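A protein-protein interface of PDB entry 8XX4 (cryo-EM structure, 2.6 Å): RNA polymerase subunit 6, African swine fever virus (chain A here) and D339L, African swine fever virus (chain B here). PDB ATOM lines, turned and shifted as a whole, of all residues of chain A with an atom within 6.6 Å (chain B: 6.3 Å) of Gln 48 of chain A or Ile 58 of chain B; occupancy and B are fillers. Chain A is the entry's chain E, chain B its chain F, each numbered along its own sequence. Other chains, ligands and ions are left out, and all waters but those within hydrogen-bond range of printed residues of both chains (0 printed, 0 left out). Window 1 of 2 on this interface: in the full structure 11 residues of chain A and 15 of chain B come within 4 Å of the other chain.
The backbone carbonyl oxygen (O) of Ser 54 of chain A lies within hydrogen-bond range of the guanidinium group (NH2) of Arg 45 of chain A (3.0 Å).
OD1 of Asn 52 of chain A sits at hydrogen-bond distance from N of Ser 54 of chain A.
The backbone NH (N) of Met 59 of chain B is in hydrogen-bond range of the backbone carbonyl oxygen (O) of Arg 66 of chain B (2.6 Å).
The side-chain hydroxyl (OG) of Ser 64 of chain B sits close to the backbone NH (N) of Arg 66 of chain B, at 3.4 Å.
Of chain B, only Pro 15, Thr 16, Ile 58 and Gly 65 come within 4 Å of Gln 48 of chain A.
Ile 58 of chain B touches just these residues of chain A: Arg 40 (3.8 Å), Val 44 (3.8 Å) and Gln 48 (3.3 Å).
Printed residues of chain B within 4 Å of Gln 47 of chain A: Ser 64 and Gly 65.
Of the printed residues of chain A, Asp 14 of chain B touches Asn 52 (3.1 Å).
Of the printed residues of chain A, Thr 16 of chain B touches Arg 45 (3.9 Å) and Gln 48 (3.8 Å).
Ser 54 of chain A touches none of the printed residues of chain B.
The nearest residue of chain B that does not touch Gln 48 of chain A is Asp 14 of chain B (5.1 Å).
The backbone carbonyl oxygen (O) of Met 59 of chain B lies within hydrogen-bond range of the guanidinium group (NH2) of Arg 40 of chain A (3.0 Å).
The side-chain amide nitrogen (NE2) of Gln 48 of chain A is in hydrogen-bond range of the backbone carbonyl oxygen (O) of Gly 65 of chain B, at 3.4 Å.
The side-chain amide nitrogen (ND2) of Asn 52 of chain A lies within hydrogen-bond range of the side-chain carboxylate (OD2) of Asp 14 of chain B (3.1 Å).
Ile 58 of chain B touches Arg 40 of chain A.
Arg 40 of chain A touches Arg 60 of chain B (NH2 to CA, 3.6 Å).
Val 44 of chain A touches Ile 58 of chain B.
Thr 16 of chain B touches Arg 45 of chain A.
Gln 47 of chain A touches Ser 64 of chain B.
Gln 47 of chain A touches Gly 65 of chain B (CG to CA, 3.7 Å).
Pro 15 of chain B touches Gln 48 of chain A (CG to NE2, 3.3 Å).
Gln 48 of chain A touches Thr 16 of chain B (OE1 to OG1, 3.8 Å).
CD1 of Ile 58 of chain B touches NE2 of Gln 48 of chain A, 3.3 Å away.
Of the 15 printed residues of chain A, 6 touch a printed residue of chain B.
Hydrophobic or aromatic side chains of chain A within 4 Å of the printed part of chain B: Val 44.
Among the printed residues, no Asp or Glu carboxylate lies within 4 Å of a Lys or Arg side-chain nitrogen of the other chain.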
ATOM      1  N   ARG A  40       6.381 -31.740  20.113  1.00  0.00           N
ATOM      2  CA  ARG A  40       6.233 -30.407  20.682  1.00  0.00           C
ATOM      3  C   ARG A  40       7.476 -29.562  20.449  1.00  0.00           C
ATOM      4  O   ARG A  40       7.371 -28.363  20.180  1.00  0.00           O
ATOM      5  CB  ARG A  40       5.935 -30.503  22.171  1.00  0.00           C
ATOM      6  CG  ARG A  40       5.959 -29.178  22.889  1.00  0.00           C
ATOM      7  CD  ARG A  40       4.656 -28.439  22.725  1.00  0.00           C
ATOM      8  NE  ARG A  40       4.584 -27.273  23.595  1.00  0.00           N
ATOM      9  CZ  ARG A  40       3.902 -26.174  23.314  1.00  0.00           C
ATOM     10  NH1 ARG A  40       3.216 -26.058  22.191  1.00  0.00           N
ATOM     11  NH2 ARG A  40       3.911 -25.166  24.177  1.00  0.00           N
ATOM     12  N   ALA A  43       7.371 -28.475  16.860  1.00  0.00           N
ATOM     13  CA  ALA A  43       6.305 -27.502  16.645  1.00  0.00           C
ATOM     14  C   ALA A  43       6.680 -26.134  17.197  1.00  0.00           C
ATOM     15  O   ALA A  43       6.476 -25.109  16.538  1.00  0.00           O
ATOM     16  CB  ALA A  43       5.010 -28.002  17.281  1.00  0.00           C
ATOM     17  N   VAL A  44       7.228 -26.097  18.413  1.00  0.00           N
ATOM     18  CA  VAL A  44       7.645 -24.835  19.011  1.00  0.00           C
ATOM     19  C   VAL A  44       8.753 -24.201  18.188  1.00  0.00           C
ATOM     20  O   VAL A  44       8.724 -22.999  17.900  1.00  0.00           O
ATOM     21  CB  VAL A  44       8.079 -25.056  20.471  1.00  0.00           C
ATOM     22  CG1 VAL A  44       8.816 -23.845  20.995  1.00  0.00           C
ATOM     23  CG2 VAL A  44       6.883 -25.354  21.334  1.00  0.00           C
ATOM     24  N   ARG A  45       9.742 -25.000  17.783  1.00  0.00           N
ATOM     25  CA  ARG A  45      10.840 -24.473  16.986  1.00  0.00           C
ATOM     26  C   ARG A  45      10.350 -23.951  15.644  1.00  0.00           C
ATOM     27  O   ARG A  45      10.806 -22.906  15.177  1.00  0.00           O
ATOM     28  CB  ARG A  45      11.901 -25.551  16.791  1.00  0.00           C
ATOM     29  CG  ARG A  45      13.174 -25.059  16.149  1.00  0.00           C
ATOM     30  CD  ARG A  45      13.651 -23.774  16.783  1.00  0.00           C
ATOM     31  NE  ARG A  45      14.828 -23.250  16.104  1.00  0.00           N
ATOM     32  CZ  ARG A  45      15.150 -21.967  16.047  1.00  0.00           C
ATOM     33  NH1 ARG A  45      14.397 -21.041  16.616  1.00  0.00           N
ATOM     34  NH2 ARG A  45      16.253 -21.604  15.404  1.00  0.00           N
ATOM     35  N   ALA A  46       9.419 -24.659  15.009  1.00  0.00           N
ATOM     36  CA  ALA A  46       8.925 -24.230  13.708  1.00  0.00           C
ATOM     37  C   ALA A  46       8.092 -22.960  13.820  1.00  0.00           C
ATOM     38  O   ALA A  46       8.199 -22.069  12.972  1.00  0.00           O
ATOM     39  CB  ALA A  46       8.126 -25.355  13.063  1.00  0.00           C
ATOM     40  N   GLN A  47       7.269 -22.843  14.862  1.00  0.00           N
ATOM     41  CA  GLN A  47       6.522 -21.604  15.053  1.00  0.00           C
ATOM     42  C   GLN A  47       7.458 -20.436  15.340  1.00  0.00           C
ATOM     43  O   GLN A  47       7.241 -19.320  14.850  1.00  0.00           O
ATOM     44  CB  GLN A  47       5.505 -21.776  16.177  1.00  0.00           C
ATOM     45  CG  GLN A  47       4.629 -20.564  16.400  1.00  0.00           C
ATOM     46  CD  GLN A  47       3.914 -20.115  15.148  1.00  0.00           C
ATOM     47  OE1 GLN A  47       4.147 -19.017  14.651  1.00  0.00           O
ATOM     48  NE2 GLN A  47       3.029 -20.960  14.636  1.00  0.00           N
ATOM     49  N   GLN A  48       8.511 -20.674  16.121  1.00  0.00           N
ATOM     50  CA  GLN A  48       9.473 -19.615  16.393  1.00  0.00           C
ATOM     51  C   GLN A  48      10.254 -19.235  15.142  1.00  0.00           C
ATOM     52  O   GLN A  48      10.598 -18.065  14.954  1.00  0.00           O
ATOM     53  CB  GLN A  48      10.407 -20.040  17.515  1.00  0.00           C
ATOM     54  CG  GLN A  48       9.747 -19.985  18.868  1.00  0.00           C
ATOM     55  CD  GLN A  48      10.602 -20.575  19.947  1.00  0.00           C
ATOM     56  OE1 GLN A  48      11.668 -21.122  19.678  1.00  0.00           O
ATOM     57  NE2 GLN A  48      10.147 -20.467  21.182  1.00  0.00           N
ATOM     58  N   LEU A  49      10.547 -20.205  14.277  1.00  0.00           N
ATOM     59  CA  LEU A  49      11.146 -19.899  12.984  1.00  0.00           C
ATOM     60  C   LEU A  49      10.161 -19.222  12.050  1.00  0.00           C
ATOM     61  O   LEU A  49      10.576 -18.643  11.044  1.00  0.00           O
ATOM     62  CB  LEU A  49      11.675 -21.168  12.325  1.00  0.00           C
ATOM     63  CG  LEU A  49      12.921 -21.806  12.927  1.00  0.00           C
ATOM     64  CD1 LEU A  49      12.916 -23.288  12.646  1.00  0.00           C
ATOM     65  CD2 LEU A  49      14.164 -21.161  12.365  1.00  0.00           C
ATOM     66  N   ALA A  50       8.866 -19.338  12.322  1.00  0.00           N
ATOM     67  CA  ALA A  50       7.888 -18.565  11.572  1.00  0.00           C
ATOM     68  C   ALA A  50       7.853 -17.115  12.039  1.00  0.00           C
ATOM     69  O   ALA A  50       7.650 -16.207  11.229  1.00  0.00           O
ATOM     70  CB  ALA A  50       6.506 -19.201  11.689  1.00  0.00           C
ATOM     71  N   ILE A  51       8.052 -16.873  13.332  1.00  0.00           N
ATOM     72  CA  ILE A  51       8.077 -15.492  13.814  1.00  0.00           C
ATOM     73  C   ILE A  51       9.475 -14.883  13.719  1.00  0.00           C
ATOM     74  O   ILE A  51       9.619 -13.708  13.380  1.00  0.00           O
ATOM     75  CB  ILE A  51       7.498 -15.405  15.243  1.00  0.00           C
ATOM     76  CG1 ILE A  51       8.432 -16.031  16.278  1.00  0.00           C
ATOM     77  CG2 ILE A  51       6.123 -16.053  15.296  1.00  0.00           C
ATOM     78  CD1 ILE A  51       7.743 -16.379  17.587  1.00  0.00           C
ATOM     79  N   ASN A  52      10.521 -15.647  14.010  1.00  0.00           N
ATOM     80  CA  ASN A  52      11.898 -15.246  13.770  1.00  0.00           C
ATOM     81  C   ASN A  52      12.335 -15.828  12.430  1.00  0.00           C
ATOM     82  O   ASN A  52      11.513 -16.285  11.637  1.00  0.00           O
ATOM     83  CB  ASN A  52      12.789 -15.699  14.929  1.00  0.00           C
ATOM     84  CG  ASN A  52      14.112 -14.960  14.979  1.00  0.00           C
ATOM     85  OD1 ASN A  52      14.921 -15.052  14.058  1.00  0.00           O
ATOM     86  ND2 ASN A  52      14.344 -14.230  16.060  1.00  0.00           N
ATOM     87  N   GLY A  53      13.631 -15.783  12.142  1.00  0.00           N
ATOM     88  CA  GLY A  53      14.120 -16.442  10.948  1.00  0.00           C
ATOM     89  C   GLY A  53      15.493 -17.061  11.094  1.00  0.00           C
ATOM     90  O   GLY A  53      16.004 -17.676  10.155  1.00  0.00           O
ATOM     91  N   SER A  54      16.094 -16.923  12.270  1.00  0.00           N
ATOM     92  CA  SER A  54      17.494 -17.273  12.463  1.00  0.00           C
ATOM     93  C   SER A  54      17.634 -18.749  12.806  1.00  0.00           C
ATOM     94  O   SER A  54      17.014 -19.237  13.755  1.00  0.00           O
ATOM     95  CB  SER A  54      18.111 -16.407  13.561  1.00  0.00           C
ATOM     96  OG  SER A  54      17.752 -16.877  14.847  1.00  0.00           O
ATOM     97  N   PRO A  78      17.334 -25.104  19.756  1.00  0.00           N
ATOM     98  CA  PRO A  78      17.674 -24.188  20.852  1.00  0.00           C
ATOM     99  C   PRO A  78      16.726 -24.276  22.035  1.00  0.00           C
ATOM    100  O   PRO A  78      16.612 -23.325  22.810  1.00  0.00           O
ATOM    101  CB  PRO A  78      17.600 -22.814  20.184  1.00  0.00           C
ATOM    102  CG  PRO A  78      16.590 -22.985  19.125  1.00  0.00           C
ATOM    103  CD  PRO A  78      16.695 -24.398  18.634  1.00  0.00           C
ATOM    104  N   LEU A  79      16.007 -25.383  22.160  1.00  0.00           N
ATOM    105  CA  LEU A  79      15.017 -25.552  23.210  1.00  0.00           C
ATOM    106  C   LEU A  79      15.484 -26.571  24.238  1.00  0.00           C
ATOM    107  O   LEU A  79      16.396 -27.361  23.998  1.00  0.00           O
ATOM    108  CB  LEU A  79      13.673 -25.986  22.623  1.00  0.00           C
ATOM    109  CG  LEU A  79      13.140 -25.119  21.488  1.00  0.00           C
ATOM    110  CD1 LEU A  79      12.117 -25.881  20.684  1.00  0.00           C
ATOM    111  CD2 LEU A  79      12.544 -23.854  22.051  1.00  0.00           C
ATOM    112  N   ASP B  14       9.282 -12.624  20.998  1.00  0.00           N
ATOM    113  CA  ASP B  14      10.350 -13.229  20.204  1.00  0.00           C
ATOM    114  C   ASP B  14      11.295 -13.936  21.163  1.00  0.00           C
ATOM    115  O   ASP B  14      12.356 -13.405  21.511  1.00  0.00           O
ATOM    116  CB  ASP B  14      11.087 -12.186  19.367  1.00  0.00           C
ATOM    117  CG  ASP B  14      11.769 -12.789  18.161  1.00  0.00           C
ATOM    118  OD1 ASP B  14      11.514 -13.976  17.870  1.00  0.00           O
ATOM    119  OD2 ASP B  14      12.556 -12.080  17.502  1.00  0.00           O
ATOM    120  N   PRO B  15      10.932 -15.134  21.621  1.00  0.00           N
ATOM    121  CA  PRO B  15      11.752 -15.809  22.638  1.00  0.00           C
ATOM    122  C   PRO B  15      13.161 -16.139  22.182  1.00  0.00           C
ATOM    123  O   PRO B  15      14.071 -16.193  23.017  1.00  0.00           O
ATOM    124  CB  PRO B  15      10.943 -17.073  22.953  1.00  0.00           C
ATOM    125  CG  PRO B  15      10.070 -17.271  21.777  1.00  0.00           C
ATOM    126  CD  PRO B  15       9.750 -15.924  21.246  1.00  0.00           C
ATOM    127  N   THR B  16      13.374 -16.372  20.886  1.00  0.00           N
ATOM    128  CA  THR B  16      14.717 -16.677  20.403  1.00  0.00           C
ATOM    129  C   THR B  16      15.640 -15.475  20.552  1.00  0.00           C
ATOM    130  O   THR B  16      16.741 -15.590  21.101  1.00  0.00           O
ATOM    131  CB  THR B  16      14.662 -17.121  18.944  1.00  0.00           C
ATOM    132  OG1 THR B  16      13.471 -17.884  18.720  1.00  0.00           O
ATOM    133  CG2 THR B  16      15.871 -17.970  18.612  1.00  0.00           C
ATOM    134  N   CYS B  56      12.506 -19.067  30.355  1.00  0.00           N
ATOM    135  CA  CYS B  56      11.520 -18.575  29.404  1.00  0.00           C
ATOM    136  C   CYS B  56      10.625 -19.717  28.950  1.00  0.00           C
ATOM    137  O   CYS B  56      10.893 -20.352  27.927  1.00  0.00           O
ATOM    138  CB  CYS B  56      12.203 -17.912  28.208  1.00  0.00           C
ATOM    139  SG  CYS B  56      11.077 -17.356  26.913  1.00  0.00           S
ATOM    140  N   PHE B  57       9.574 -19.996  29.713  1.00  0.00           N
ATOM    141  CA  PHE B  57       8.645 -21.054  29.348  1.00  0.00           C
ATOM    142  C   PHE B  57       7.895 -20.685  28.079  1.00  0.00           C
ATOM    143  O   PHE B  57       7.454 -19.551  27.914  1.00  0.00           O
ATOM    144  CB  PHE B  57       7.640 -21.298  30.467  1.00  0.00           C
ATOM    145  CG  PHE B  57       8.255 -21.472  31.815  1.00  0.00           C
ATOM    146  CD1 PHE B  57       8.916 -22.634  32.141  1.00  0.00           C
ATOM    147  CD2 PHE B  57       8.148 -20.483  32.768  1.00  0.00           C
ATOM    148  CE1 PHE B  57       9.472 -22.798  33.381  1.00  0.00           C
ATOM    149  CE2 PHE B  57       8.702 -20.647  34.011  1.00  0.00           C
ATOM    150  CZ  PHE B  57       9.366 -21.807  34.316  1.00  0.00           C
ATOM    151  N   ILE B  58       7.739 -21.649  27.191  1.00  0.00           N
ATOM    152  CA  ILE B  58       6.948 -21.444  25.986  1.00  0.00           C
ATOM    153  C   ILE B  58       5.474 -21.534  26.342  1.00  0.00           C
ATOM    154  O   ILE B  58       5.057 -22.420  27.095  1.00  0.00           O
ATOM    155  CB  ILE B  58       7.332 -22.469  24.907  1.00  0.00           C
ATOM    156  CG1 ILE B  58       8.782 -22.263  24.480  1.00  0.00           C
ATOM    157  CG2 ILE B  58       6.419 -22.349  23.708  1.00  0.00           C
ATOM    158  CD1 ILE B  58       9.143 -20.826  24.286  1.00  0.00           C
ATOM    159  N   MET B  59       4.681 -20.603  25.818  1.00  0.00           N
ATOM    160  CA  MET B  59       3.249 -20.605  26.076  1.00  0.00           C
ATOM    161  C   MET B  59       2.637 -21.919  25.616  1.00  0.00           C
ATOM    162  O   MET B  59       2.919 -22.399  24.515  1.00  0.00           O
ATOM    163  CB  MET B  59       2.586 -19.432  25.366  1.00  0.00           C
ATOM    164  CG  MET B  59       2.900 -18.095  25.983  1.00  0.00           C
ATOM    165  SD  MET B  59       2.092 -16.731  25.143  1.00  0.00           S
ATOM    166  CE  MET B  59       2.578 -15.373  26.192  1.00  0.00           C
ATOM    167  N   ARG B  60       1.801 -22.500  26.463  1.00  0.00           N
ATOM    168  CA  ARG B  60       1.267 -23.835  26.247  1.00  0.00           C
ATOM    169  C   ARG B  60      -0.176 -23.843  25.779  1.00  0.00           C
ATOM    170  O   ARG B  60      -0.577 -24.749  25.050  1.00  0.00           O
ATOM    171  CB  ARG B  60       1.387 -24.652  27.538  1.00  0.00           C
ATOM    172  CG  ARG B  60       0.935 -26.083  27.421  1.00  0.00           C
ATOM    173  CD  ARG B  60       0.870 -26.741  28.780  1.00  0.00           C
ATOM    174  NE  ARG B  60      -0.175 -26.162  29.612  1.00  0.00           N
ATOM    175  CZ  ARG B  60      -1.457 -26.491  29.544  1.00  0.00           C
ATOM    176  NH1 ARG B  60      -1.894 -27.393  28.686  1.00  0.00           N
ATOM    177  NH2 ARG B  60      -2.322 -25.898  30.360  1.00  0.00           N
ATOM    178  N   THR B  61      -0.968 -22.848  26.164  1.00  0.00           N
ATOM    179  CA  THR B  61      -2.388 -22.844  25.850  1.00  0.00           C
ATOM    180  C   THR B  61      -2.714 -22.134  24.544  1.00  0.00           C
ATOM    181  O   THR B  61      -3.895 -21.964  24.234  1.00  0.00           O
ATOM    182  CB  THR B  61      -3.175 -22.208  26.992  1.00  0.00           C
ATOM    183  OG1 THR B  61      -2.533 -20.996  27.397  1.00  0.00           O
ATOM    184  CG2 THR B  61      -3.238 -23.157  28.173  1.00  0.00           C
ATOM    185  N   SER B  64       0.958 -19.809  19.583  1.00  0.00           N
ATOM    186  CA  SER B  64       1.685 -18.621  19.161  1.00  0.00           C
ATOM    187  C   SER B  64       3.187 -18.843  19.116  1.00  0.00           C
ATOM    188  O   SER B  64       3.881 -18.175  18.346  1.00  0.00           O
ATOM    189  CB  SER B  64       1.370 -17.455  20.093  1.00  0.00           C
ATOM    190  OG  SER B  64       1.755 -17.753  21.420  1.00  0.00           O
ATOM    191  N   GLY B  65       3.705 -19.760  19.926  1.00  0.00           N
ATOM    192  CA  GLY B  65       5.135 -19.962  20.006  1.00  0.00           C
ATOM    193  C   GLY B  65       5.863 -18.981  20.891  1.00  0.00           C
ATOM    194  O   GLY B  65       7.096 -18.997  20.919  1.00  0.00           O
ATOM    195  N   ARG B  66       5.142 -18.131  21.612  1.00  0.00           N
ATOM    196  CA  ARG B  66       5.747 -17.124  22.466  1.00  0.00           C
ATOM    197  C   ARG B  66       6.078 -17.703  23.836  1.00  0.00           C
ATOM    198  O   ARG B  66       5.581 -18.755  24.236  1.00  0.00           O
ATOM    199  CB  ARG B  66       4.814 -15.927  22.615  1.00  0.00           C
ATOM    200  CG  ARG B  66       4.671 -15.091  21.371  1.00  0.00           C
ATOM    201  CD  ARG B  66       3.262 -14.562  21.240  1.00  0.00           C
ATOM    202  NE  ARG B  66       2.918 -13.626  22.303  1.00  0.00           N
ATOM    203  CZ  ARG B  66       1.718 -13.539  22.861  1.00  0.00           C
ATOM    204  NH1 ARG B  66       0.725 -14.331  22.492  1.00  0.00           N
ATOM    205  NH2 ARG B  66       1.510 -12.632  23.810  1.00  0.00           N
ATOM    206  N   GLY B  67       6.937 -16.995  24.560  1.00  0.00           N
ATOM    207  CA  GLY B  67       7.293 -17.371  25.912  1.00  0.00           C
ATOM    208  C   GLY B  67       6.845 -16.317  26.894  1.00  0.00           C
ATOM    209  O   GLY B  67       6.483 -15.219  26.467  1.00  0.00           O
ATOM    210  N   TYR B  68       6.829 -16.605  28.195  1.00  0.00           N
ATOM    211  CA  TYR B  68       6.400 -15.584  29.144  1.00  0.00           C
ATOM    212  C   TYR B  68       7.477 -15.188  30.146  1.00  0.00           C
ATOM    213  O   TYR B  68       7.804 -14.000  30.222  1.00  0.00           O
ATOM    214  CB  TYR B  68       5.110 -15.994  29.870  1.00  0.00           C
ATOM    215  CG  TYR B  68       4.967 -17.431  30.304  1.00  0.00           C
ATOM    216  CD1 TYR B  68       4.662 -18.429  29.392  1.00  0.00           C
ATOM    217  CD2 TYR B  68       5.062 -17.774  31.639  1.00  0.00           C
ATOM    218  CE1 TYR B  68       4.501 -19.728  29.794  1.00  0.00           C
ATOM    219  CE2 TYR B  68       4.901 -19.069  32.046  1.00  0.00           C
ATOM    220  CZ  TYR B  68       4.618 -20.041  31.121  1.00  0.00           C
ATOM    221  OH  TYR B  68       4.457 -21.339  31.529  1.00  0.00           O
